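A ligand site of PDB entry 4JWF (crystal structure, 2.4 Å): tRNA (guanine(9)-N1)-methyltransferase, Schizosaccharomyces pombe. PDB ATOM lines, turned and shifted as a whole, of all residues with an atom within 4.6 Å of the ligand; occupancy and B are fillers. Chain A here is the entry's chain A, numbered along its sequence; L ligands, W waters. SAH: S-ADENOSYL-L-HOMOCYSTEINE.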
ATOM      1  N   TYR A 118     -19.593 -16.397 -11.449  1.00  0.00           N
ATOM      2  CA  TYR A 118     -18.374 -16.839 -12.105  1.00  0.00           C
ATOM      3  C   TYR A 118     -17.849 -18.085 -11.430  1.00  0.00           C
ATOM      4  O   TYR A 118     -17.462 -18.050 -10.276  1.00  0.00           O
ATOM      5  CB  TYR A 118     -17.316 -15.728 -12.062  1.00  0.00           C
ATOM      6  CG  TYR A 118     -16.390 -15.721 -13.265  1.00  0.00           C
ATOM      7  CD1 TYR A 118     -16.319 -14.593 -14.088  1.00  0.00           C
ATOM      8  CD2 TYR A 118     -15.582 -16.828 -13.569  1.00  0.00           C
ATOM      9  CE1 TYR A 118     -15.469 -14.564 -15.193  1.00  0.00           C
ATOM     10  CE2 TYR A 118     -14.736 -16.813 -14.689  1.00  0.00           C
ATOM     11  CZ  TYR A 118     -14.685 -15.671 -15.491  1.00  0.00           C
ATOM     12  OH  TYR A 118     -13.854 -15.627 -16.573  1.00  0.00           O
ATOM     13  N   LEU A 119     -17.842 -19.203 -12.151  1.00  0.00           N
ATOM     14  CA  LEU A 119     -17.264 -20.413 -11.611  1.00  0.00           C
ATOM     15  C   LEU A 119     -15.760 -20.288 -11.557  1.00  0.00           C
ATOM     16  O   LEU A 119     -15.128 -19.873 -12.533  1.00  0.00           O
ATOM     17  CB  LEU A 119     -17.690 -21.624 -12.439  1.00  0.00           C
ATOM     18  CG  LEU A 119     -19.183 -21.909 -12.440  1.00  0.00           C
ATOM     19  CD1 LEU A 119     -19.511 -22.956 -13.483  1.00  0.00           C
ATOM     20  CD2 LEU A 119     -19.669 -22.372 -11.058  1.00  0.00           C
ATOM     21  N   SER A 120     -15.186 -20.598 -10.397  1.00  0.00           N
ATOM     22  CA  SER A 120     -13.733 -20.548 -10.222  1.00  0.00           C
ATOM     23  C   SER A 120     -13.291 -21.545  -9.167  1.00  0.00           C
ATOM     24  O   SER A 120     -13.924 -21.670  -8.136  1.00  0.00           O
ATOM     25  CB  SER A 120     -13.278 -19.140  -9.815  1.00  0.00           C
ATOM     26  OG  SER A 120     -11.918 -19.165  -9.391  1.00  0.00           O
ATOM     27  N   ALA A 121     -12.194 -22.235  -9.430  1.00  0.00           N
ATOM     28  CA  ALA A 121     -11.634 -23.175  -8.471  1.00  0.00           C
ATOM     29  C   ALA A 121     -11.032 -22.456  -7.251  1.00  0.00           C
ATOM     30  O   ALA A 121     -10.740 -23.084  -6.252  1.00  0.00           O
ATOM     31  CB  ALA A 121     -10.596 -24.042  -9.140  1.00  0.00           C
ATOM     32  N   ASP A 122     -10.852 -21.137  -7.355  1.00  0.00           N
ATOM     33  CA  ASP A 122     -10.197 -20.340  -6.314  1.00  0.00           C
ATOM     34  C   ASP A 122     -11.212 -19.642  -5.390  1.00  0.00           C
ATOM     35  O   ASP A 122     -10.842 -18.835  -4.545  1.00  0.00           O
ATOM     36  CB  ASP A 122      -9.274 -19.270  -6.938  1.00  0.00           C
ATOM     37  CG  ASP A 122      -8.168 -19.861  -7.817  1.00  0.00           C
ATOM     38  OD1 ASP A 122      -7.316 -20.614  -7.307  1.00  0.00           O
ATOM     39  OD2 ASP A 122      -8.128 -19.534  -9.020  1.00  0.00           O
ATOM     40  N   ILE A 137     -20.784 -18.443 -15.434  1.00  0.00           N
ATOM     41  CA  ILE A 137     -19.685 -18.071 -16.306  1.00  0.00           C
ATOM     42  C   ILE A 137     -18.541 -19.048 -16.154  1.00  0.00           C
ATOM     43  O   ILE A 137     -18.136 -19.372 -15.025  1.00  0.00           O
ATOM     44  CB  ILE A 137     -19.191 -16.636 -16.009  1.00  0.00           C
ATOM     45  CG1 ILE A 137     -20.366 -15.642 -16.120  1.00  0.00           C
ATOM     46  CG2 ILE A 137     -18.037 -16.250 -16.945  1.00  0.00           C
ATOM     47  CD1 ILE A 137     -20.140 -14.325 -15.370  1.00  0.00           C
ATOM     48  N   ILE A 138     -18.033 -19.517 -17.291  1.00  0.00           N
ATOM     49  CA  ILE A 138     -16.834 -20.336 -17.336  1.00  0.00           C
ATOM     50  C   ILE A 138     -15.756 -19.534 -18.037  1.00  0.00           C
ATOM     51  O   ILE A 138     -15.970 -19.021 -19.142  1.00  0.00           O
ATOM     52  CB  ILE A 138     -17.075 -21.679 -18.064  1.00  0.00           C
ATOM     53  CG1 ILE A 138     -18.327 -22.379 -17.537  1.00  0.00           C
ATOM     54  CG2 ILE A 138     -15.856 -22.591 -17.928  1.00  0.00           C
ATOM     55  CD1 ILE A 138     -18.745 -23.643 -18.323  1.00  0.00           C
ATOM     56  N   GLY A 139     -14.596 -19.388 -17.390  1.00  0.00           N
ATOM     57  CA  GLY A 139     -13.483 -18.665 -17.995  1.00  0.00           C
ATOM     58  C   GLY A 139     -12.996 -19.446 -19.191  1.00  0.00           C
ATOM     59  O   GLY A 139     -12.593 -20.606 -19.062  1.00  0.00           O
ATOM     60  N   ILE A 141     -10.384 -20.198 -21.018  1.00  0.00           N
ATOM     61  CA  ILE A 141      -8.915 -20.181 -21.053  1.00  0.00           C
ATOM     62  C   ILE A 141      -8.289 -21.547 -20.765  1.00  0.00           C
ATOM     63  O   ILE A 141      -8.745 -22.297 -19.882  1.00  0.00           O
ATOM     64  CB  ILE A 141      -8.329 -19.070 -20.136  1.00  0.00           C
ATOM     65  CG1 ILE A 141      -6.839 -18.858 -20.419  1.00  0.00           C
ATOM     66  CG2 ILE A 141      -8.643 -19.337 -18.658  1.00  0.00           C
ATOM     67  CD1 ILE A 141      -6.194 -17.740 -19.643  1.00  0.00           C
ATOM     68  N   ASP A 143      -4.837 -22.570 -19.512  1.00  0.00           N
ATOM     69  CA  ASP A 143      -3.605 -22.055 -18.930  1.00  0.00           C
ATOM     70  C   ASP A 143      -2.898 -23.097 -18.056  1.00  0.00           C
ATOM     71  O   ASP A 143      -1.867 -22.797 -17.440  1.00  0.00           O
ATOM     72  CB  ASP A 143      -3.894 -20.798 -18.103  1.00  0.00           C
ATOM     73  CG  ASP A 143      -4.663 -21.096 -16.827  1.00  0.00           C
ATOM     74  OD1 ASP A 143      -5.401 -22.097 -16.775  1.00  0.00           O
ATOM     75  OD2 ASP A 143      -4.535 -20.309 -15.876  1.00  0.00           O
ATOM     76  N   ASN A 145      -3.803 -23.883 -15.340  1.00  0.00           N
ATOM     77  CA  ASN A 145      -3.845 -23.167 -14.044  1.00  0.00           C
ATOM     78  C   ASN A 145      -2.578 -22.353 -13.705  1.00  0.00           C
ATOM     79  O   ASN A 145      -2.331 -21.999 -12.544  1.00  0.00           O
ATOM     80  CB  ASN A 145      -4.258 -24.110 -12.899  1.00  0.00           C
ATOM     81  CG  ASN A 145      -4.813 -23.357 -11.704  1.00  0.00           C
ATOM     82  OD1 ASN A 145      -5.617 -22.438 -11.853  1.00  0.00           O
ATOM     83  ND2 ASN A 145      -4.370 -23.738 -10.514  1.00  0.00           N
ATOM     84  N   TYR A 147      -2.159 -19.248 -14.424  1.00  0.00           N
ATOM     85  CA  TYR A 147      -2.648 -17.979 -13.868  1.00  0.00           C
ATOM     86  C   TYR A 147      -3.695 -18.257 -12.780  1.00  0.00           C
ATOM     87  O   TYR A 147      -4.903 -18.105 -12.996  1.00  0.00           O
ATOM     88  CB  TYR A 147      -3.239 -17.076 -14.965  1.00  0.00           C
ATOM     89  CG  TYR A 147      -2.428 -16.974 -16.233  1.00  0.00           C
ATOM     90  CD1 TYR A 147      -1.153 -16.404 -16.246  1.00  0.00           C
ATOM     91  CD2 TYR A 147      -2.959 -17.441 -17.432  1.00  0.00           C
ATOM     92  CE1 TYR A 147      -0.418 -16.304 -17.449  1.00  0.00           C
ATOM     93  CE2 TYR A 147      -2.252 -17.349 -18.614  1.00  0.00           C
ATOM     94  CZ  TYR A 147      -0.990 -16.779 -18.631  1.00  0.00           C
ATOM     95  OH  TYR A 147      -0.323 -16.705 -19.835  1.00  0.00           O
ATOM     96  N   LYS A 148      -3.197 -18.667 -11.609  1.00  0.00           N
ATOM     97  CA  LYS A 148      -4.055 -18.863 -10.440  1.00  0.00           C
ATOM     98  C   LYS A 148      -4.693 -17.531 -10.079  1.00  0.00           C
ATOM     99  O   LYS A 148      -4.056 -16.491 -10.209  1.00  0.00           O
ATOM    100  CB  LYS A 148      -3.239 -19.423  -9.267  1.00  0.00           C
ATOM    101  N   ASN A 149      -5.952 -17.585  -9.654  1.00  0.00           N
ATOM    102  CA  ASN A 149      -6.755 -16.414  -9.267  1.00  0.00           C
ATOM    103  C   ASN A 149      -7.205 -15.447 -10.354  1.00  0.00           C
ATOM    104  O   ASN A 149      -7.875 -14.451 -10.075  1.00  0.00           O
ATOM    105  CB  ASN A 149      -6.124 -15.660  -8.093  1.00  0.00           C
ATOM    106  CG  ASN A 149      -6.709 -16.082  -6.767  1.00  0.00           C
ATOM    107  OD1 ASN A 149      -7.801 -15.636  -6.395  1.00  0.00           O
ATOM    108  ND2 ASN A 149      -6.019 -16.964  -6.063  1.00  0.00           N
ATOM    109  N   LEU A 150      -6.868 -15.753 -11.604  1.00  0.00           N
ATOM    110  CA  LEU A 150      -7.263 -14.901 -12.710  1.00  0.00           C
ATOM    111  C   LEU A 150      -8.764 -14.600 -12.690  1.00  0.00           C
ATOM    112  O   LEU A 150      -9.182 -13.443 -12.682  1.00  0.00           O
ATOM    113  CB  LEU A 150      -6.877 -15.552 -14.044  1.00  0.00           C
ATOM    114  CG  LEU A 150      -7.251 -14.799 -15.312  1.00  0.00           C
ATOM    115  CD1 LEU A 150      -6.417 -13.533 -15.437  1.00  0.00           C
ATOM    116  CD2 LEU A 150      -7.087 -15.720 -16.518  1.00  0.00           C
ATOM    117  N   CYS A 151      -9.566 -15.654 -12.659  1.00  0.00           N
ATOM    118  CA  CYS A 151     -11.010 -15.511 -12.760  1.00  0.00           C
ATOM    119  C   CYS A 151     -11.667 -15.058 -11.453  1.00  0.00           C
ATOM    120  O   CYS A 151     -12.578 -14.220 -11.467  1.00  0.00           O
ATOM    121  CB  CYS A 151     -11.621 -16.786 -13.319  1.00  0.00           C
ATOM    122  SG  CYS A 151     -11.084 -17.057 -15.040  1.00  0.00           S
ATOM    123  N   ALA A 163     -17.945 -19.180  -7.306  1.00  0.00           N
ATOM    124  CA  ALA A 163     -18.189 -20.471  -6.676  1.00  0.00           C
ATOM    125  C   ALA A 163     -17.346 -21.534  -7.354  1.00  0.00           C
ATOM    126  O   ALA A 163     -17.157 -21.520  -8.565  1.00  0.00           O
ATOM    127  CB  ALA A 163     -19.666 -20.832  -6.761  1.00  0.00           C
ATOM    128  N   LYS A 164     -16.832 -22.461  -6.551  1.00  0.00           N
ATOM    129  CA  LYS A 164     -16.141 -23.625  -7.070  1.00  0.00           C
ATOM    130  C   LYS A 164     -17.082 -24.835  -7.138  1.00  0.00           C
ATOM    131  O   LYS A 164     -18.126 -24.848  -6.490  1.00  0.00           O
ATOM    132  CB  LYS A 164     -14.897 -23.938  -6.231  1.00  0.00           C
ATOM    133  CG  LYS A 164     -15.139 -24.186  -4.769  1.00  0.00           C
ATOM    134  CD  LYS A 164     -13.828 -24.189  -3.987  1.00  0.00           C
ATOM    135  CE  LYS A 164     -14.054 -24.475  -2.513  1.00  0.00           C
ATOM    136  NZ  LYS A 164     -12.774 -24.894  -1.864  1.00  0.00           N
ATOM    137  N   LEU A 165     -16.705 -25.812  -7.943  1.00  0.00           N
ATOM    138  CA  LEU A 165     -17.459 -27.065  -8.038  1.00  0.00           C
ATOM    139  C   LEU A 165     -17.278 -27.915  -6.785  1.00  0.00           C
ATOM    140  O   LEU A 165     -16.194 -27.955  -6.208  1.00  0.00           O
ATOM    141  CB  LEU A 165     -17.034 -27.854  -9.278  1.00  0.00           C
ATOM    142  CG  LEU A 165     -17.434 -27.354 -10.683  1.00  0.00           C
ATOM    143  CD1 LEU A 165     -16.827 -28.272 -11.733  1.00  0.00           C
ATOM    144  CD2 LEU A 165     -18.942 -27.289 -10.839  1.00  0.00           C
ATOM    145  N   ILE A 167     -16.434 -30.659  -6.087  1.00  0.00           N
ATOM    146  CA  ILE A 167     -15.512 -31.792  -6.167  1.00  0.00           C
ATOM    147  C   ILE A 167     -14.631 -31.681  -4.919  1.00  0.00           C
ATOM    148  O   ILE A 167     -14.727 -30.683  -4.200  1.00  0.00           O
ATOM    149  CB  ILE A 167     -14.701 -31.825  -7.501  1.00  0.00           C
ATOM    150  CG1 ILE A 167     -13.427 -30.993  -7.435  1.00  0.00           C
ATOM    151  CG2 ILE A 167     -15.541 -31.349  -8.659  1.00  0.00           C
ATOM    152  CD1 ILE A 167     -12.578 -31.134  -8.692  1.00  0.00           C
ATOM    153  N   LYS A 177      -7.816 -30.331  -8.964  1.00  0.00           N
ATOM    154  CA  LYS A 177      -9.220 -29.978  -8.880  1.00  0.00           C
ATOM    155  C   LYS A 177      -9.639 -28.925  -9.925  1.00  0.00           C
ATOM    156  O   LYS A 177     -10.777 -28.461  -9.932  1.00  0.00           O
ATOM    157  CB  LYS A 177      -9.541 -29.469  -7.468  1.00  0.00           C
ATOM    158  N   ILE A 178      -8.700 -28.553 -10.799  1.00  0.00           N
ATOM    159  CA  ILE A 178      -8.960 -27.567 -11.853  1.00  0.00           C
ATOM    160  C   ILE A 178      -9.203 -28.244 -13.199  1.00  0.00           C
ATOM    161  O   ILE A 178      -8.297 -28.810 -13.814  1.00  0.00           O
ATOM    162  CB  ILE A 178      -7.826 -26.510 -11.972  1.00  0.00           C
ATOM    163  CG1 ILE A 178      -7.549 -25.847 -10.622  1.00  0.00           C
ATOM    164  CG2 ILE A 178      -8.196 -25.453 -13.008  1.00  0.00           C
ATOM    165  CD1 ILE A 178      -6.439 -26.496  -9.808  1.00  0.00           C
ATOM    166  N   LEU A 179     -10.452 -28.167 -13.638  1.00  0.00           N
ATOM    167  CA  LEU A 179     -10.910 -28.858 -14.841  1.00  0.00           C
ATOM    168  C   LEU A 179     -10.809 -27.987 -16.099  1.00  0.00           C
ATOM    169  O   LEU A 179     -10.636 -26.774 -16.010  1.00  0.00           O
ATOM    170  CB  LEU A 179     -12.330 -29.338 -14.619  1.00  0.00           C
ATOM    171  CG  LEU A 179     -12.553 -30.055 -13.274  1.00  0.00           C
ATOM    172  CD1 LEU A 179     -14.016 -30.317 -13.050  1.00  0.00           C
ATOM    173  CD2 LEU A 179     -11.755 -31.356 -13.177  1.00  0.00           C
ATOM    174  N   VAL A 181     -12.477 -26.354 -19.672  1.00  0.00           N
ATOM    175  CA  VAL A 181     -13.727 -25.639 -19.964  1.00  0.00           C
ATOM    176  C   VAL A 181     -14.872 -26.611 -20.250  1.00  0.00           C
ATOM    177  O   VAL A 181     -15.909 -26.547 -19.606  1.00  0.00           O
ATOM    178  CB  VAL A 181     -13.558 -24.637 -21.137  1.00  0.00           C
ATOM    179  CG1 VAL A 181     -14.908 -24.163 -21.670  1.00  0.00           C
ATOM    180  CG2 VAL A 181     -12.715 -23.455 -20.708  1.00  0.00           C
ATOM    181  N   VAL A 184     -16.155 -28.745 -17.159  1.00  0.00           N
ATOM    182  CA  VAL A 184     -16.998 -27.979 -16.255  1.00  0.00           C
ATOM    183  C   VAL A 184     -18.394 -27.834 -16.843  1.00  0.00           C
ATOM    184  O   VAL A 184     -19.396 -28.035 -16.155  1.00  0.00           O
ATOM    185  CB  VAL A 184     -16.401 -26.584 -15.947  1.00  0.00           C
ATOM    186  CG1 VAL A 184     -17.349 -25.763 -15.073  1.00  0.00           C
ATOM    187  CG2 VAL A 184     -15.030 -26.725 -15.263  1.00  0.00           C
HETATM  188  N   SAH L   1      -6.320 -20.188 -14.024  1.00  0.00           N
HETATM  189  CA  SAH L   1      -7.719 -20.269 -14.551  1.00  0.00           C
HETATM  190  CB  SAH L   1      -8.154 -21.738 -14.632  1.00  0.00           C
HETATM  191  CG  SAH L   1      -8.638 -22.089 -16.033  1.00  0.00           C
HETATM  192  SD  SAH L   1      -9.613 -23.570 -16.046  1.00  0.00           S
HETATM  193  C   SAH L   1      -8.620 -19.473 -13.641  1.00  0.00           C
HETATM  194  O   SAH L   1      -8.170 -18.566 -12.935  1.00  0.00           O
HETATM  195  OXT SAH L   1      -9.830 -19.687 -13.559  1.00  0.00           O
HETATM  196  C5' SAH L   1     -10.950 -23.032 -17.083  1.00  0.00           C
HETATM  197  C4' SAH L   1     -12.211 -22.500 -16.357  1.00  0.00           C
HETATM  198  O4' SAH L   1     -13.035 -23.568 -15.885  1.00  0.00           O
HETATM  199  C3' SAH L   1     -11.990 -21.583 -15.165  1.00  0.00           C
HETATM  200  O3' SAH L   1     -11.988 -20.216 -15.555  1.00  0.00           O
HETATM  201  C2' SAH L   1     -13.165 -21.842 -14.255  1.00  0.00           C
HETATM  202  O2' SAH L   1     -14.267 -20.994 -14.573  1.00  0.00           O
HETATM  203  C1' SAH L   1     -13.616 -23.228 -14.615  1.00  0.00           C
HETATM  204  N9  SAH L   1     -13.191 -24.205 -13.574  1.00  0.00           N
HETATM  205  C8  SAH L   1     -12.176 -25.089 -13.662  1.00  0.00           C
HETATM  206  N7  SAH L   1     -12.094 -25.863 -12.541  1.00  0.00           N
HETATM  207  C5  SAH L   1     -13.080 -25.453 -11.723  1.00  0.00           C
HETATM  208  C6  SAH L   1     -13.580 -25.834 -10.376  1.00  0.00           C
HETATM  209  N6  SAH L   1     -12.978 -26.819  -9.672  1.00  0.00           N
HETATM  210  N1  SAH L   1     -14.639 -25.164  -9.874  1.00  0.00           N
HETATM  211  C2  SAH L   1     -15.263 -24.177 -10.549  1.00  0.00           C
HETATM  212  N3  SAH L   1     -14.867 -23.782 -11.777  1.00  0.00           N
HETATM  213  C4  SAH L   1     -13.798 -24.370 -12.401  1.00  0.00           C
HETATM  214  O   HOH W   1      -9.697 -17.998 -10.465  1.00  0.00           O
HETATM  215  O   HOH W   2     -13.684 -26.902  -6.741  1.00  0.00           O
HETATM  216  O   HOH W   3     -10.778 -21.804 -11.763  1.00  0.00           O
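O of Leu 119 sits at hydrogen-bond distance from O2' of the ligand, 2.5 Å away. The side-chain carboxylate (OD2) of Asp 143 is in salt-bridge range of a nitrogen (N) of the ligand, at 2.6 Å. A nitrogen (N) of the ligand sits at hydrogen-bond distance from the backbone carbonyl oxygen (O) of Tyr 147 (2.7 Å). N6 of the ligand lies within hydrogen-bond range of O of Lys 177, at 2.8 Å. N1 of the ligand lies within hydrogen-bond range of N of Leu 165. N of Leu 179 lies within hydrogen-bond range of N7 of the ligand. A nitrogen (N) of the ligand lies within hydrogen-bond range of the side-chain amide oxygen (OD1) of Asn 145 (3.2 Å). The backbone NH of Cys 151 lies within hydrogen-bond range of an oxygen (O) of the ligand (3.2 Å). OXT of the ligand lies within hydrogen-bond range of SG of Cys 151, 3.3 Å away. N of Gly 139 sits at hydrogen-bond distance from O2' of the ligand, at 3.3 Å. N of Leu 150 lies within hydrogen-bond range of O of the ligand (3.4 Å). N of Ser 120 is in hydrogen-bond range of N3 of the ligand.
The backbone NH (N) of Leu 119 sits at hydrogen-bond distance from the backbone carbonyl oxygen (O) of Ile 137 (2.9 Å). OD2 of Asp 143 lies within hydrogen-bond range of N of Tyr 147 (3.0 Å). The backbone NH (N) of Asn 145 is in hydrogen-bond range of the side-chain carboxylate (OD1) of Asp 143, at 2.8 Å. The side-chain sulfur (SG) of Cys 151 lies within hydrogen-bond range of the side-chain hydroxyl (OH) of Tyr 118 (3.5 Å). The backbone carbonyl oxygen (O) of Ser 120 lies close to the backbone NH (N) of Lys 164 (3.4 Å). N of Ser 120 lies within hydrogen-bond range of O of Ala 163 (2.8 Å). The side-chain hydroxyl of Ser 120 sits at hydrogen-bond distance from the backbone NH of Asp 122, at 3.0 Å. N of Ala 163 lies within hydrogen-bond range of O of Tyr 118 (3.2 Å).
CB of Ala 121 touches C6 of the ligand (3.7 Å). Ile 138 touches the ligand (CG2 to O4', 3.6 Å). Ile 141 touches the ligand (O to C5', 3.6 Å). Ala 163 touches the ligand (O to C2, 3.8 Å). CA of Lys 164 touches N1 of the ligand (3.5 Å). Ile 178 touches the ligand. Val 184 touches the ligand. Hydrophobic or aromatic side chains within 4 Å of the ligand: Leu 119, Ala 121, Ile 138, Ile 141, Leu 150, Leu 165, Ile 178 and Val 184. Of the 25 residues printed, 18 come within 4 Å of the ligand. The nearest printed residue that does not touch the ligand is Asp 122 (4.03 Å).
Water W3 bridges N of Ala 121 (2.8 Å) and OXT of the ligand (2.9 Å). Water W1 lies within hydrogen-bond range of OD2 of Asp 122 (2.6 Å), OG of Ser 120 (2.7 Å), O of the ligand (3.0 Å) and N of Cys 151 (3.2 Å). Water W2 lies within hydrogen-bond range of the backbone carbonyl oxygen (O) of Leu 165 (2.8 Å) and a nitrogen (N6) of the ligand (3.0 Å).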
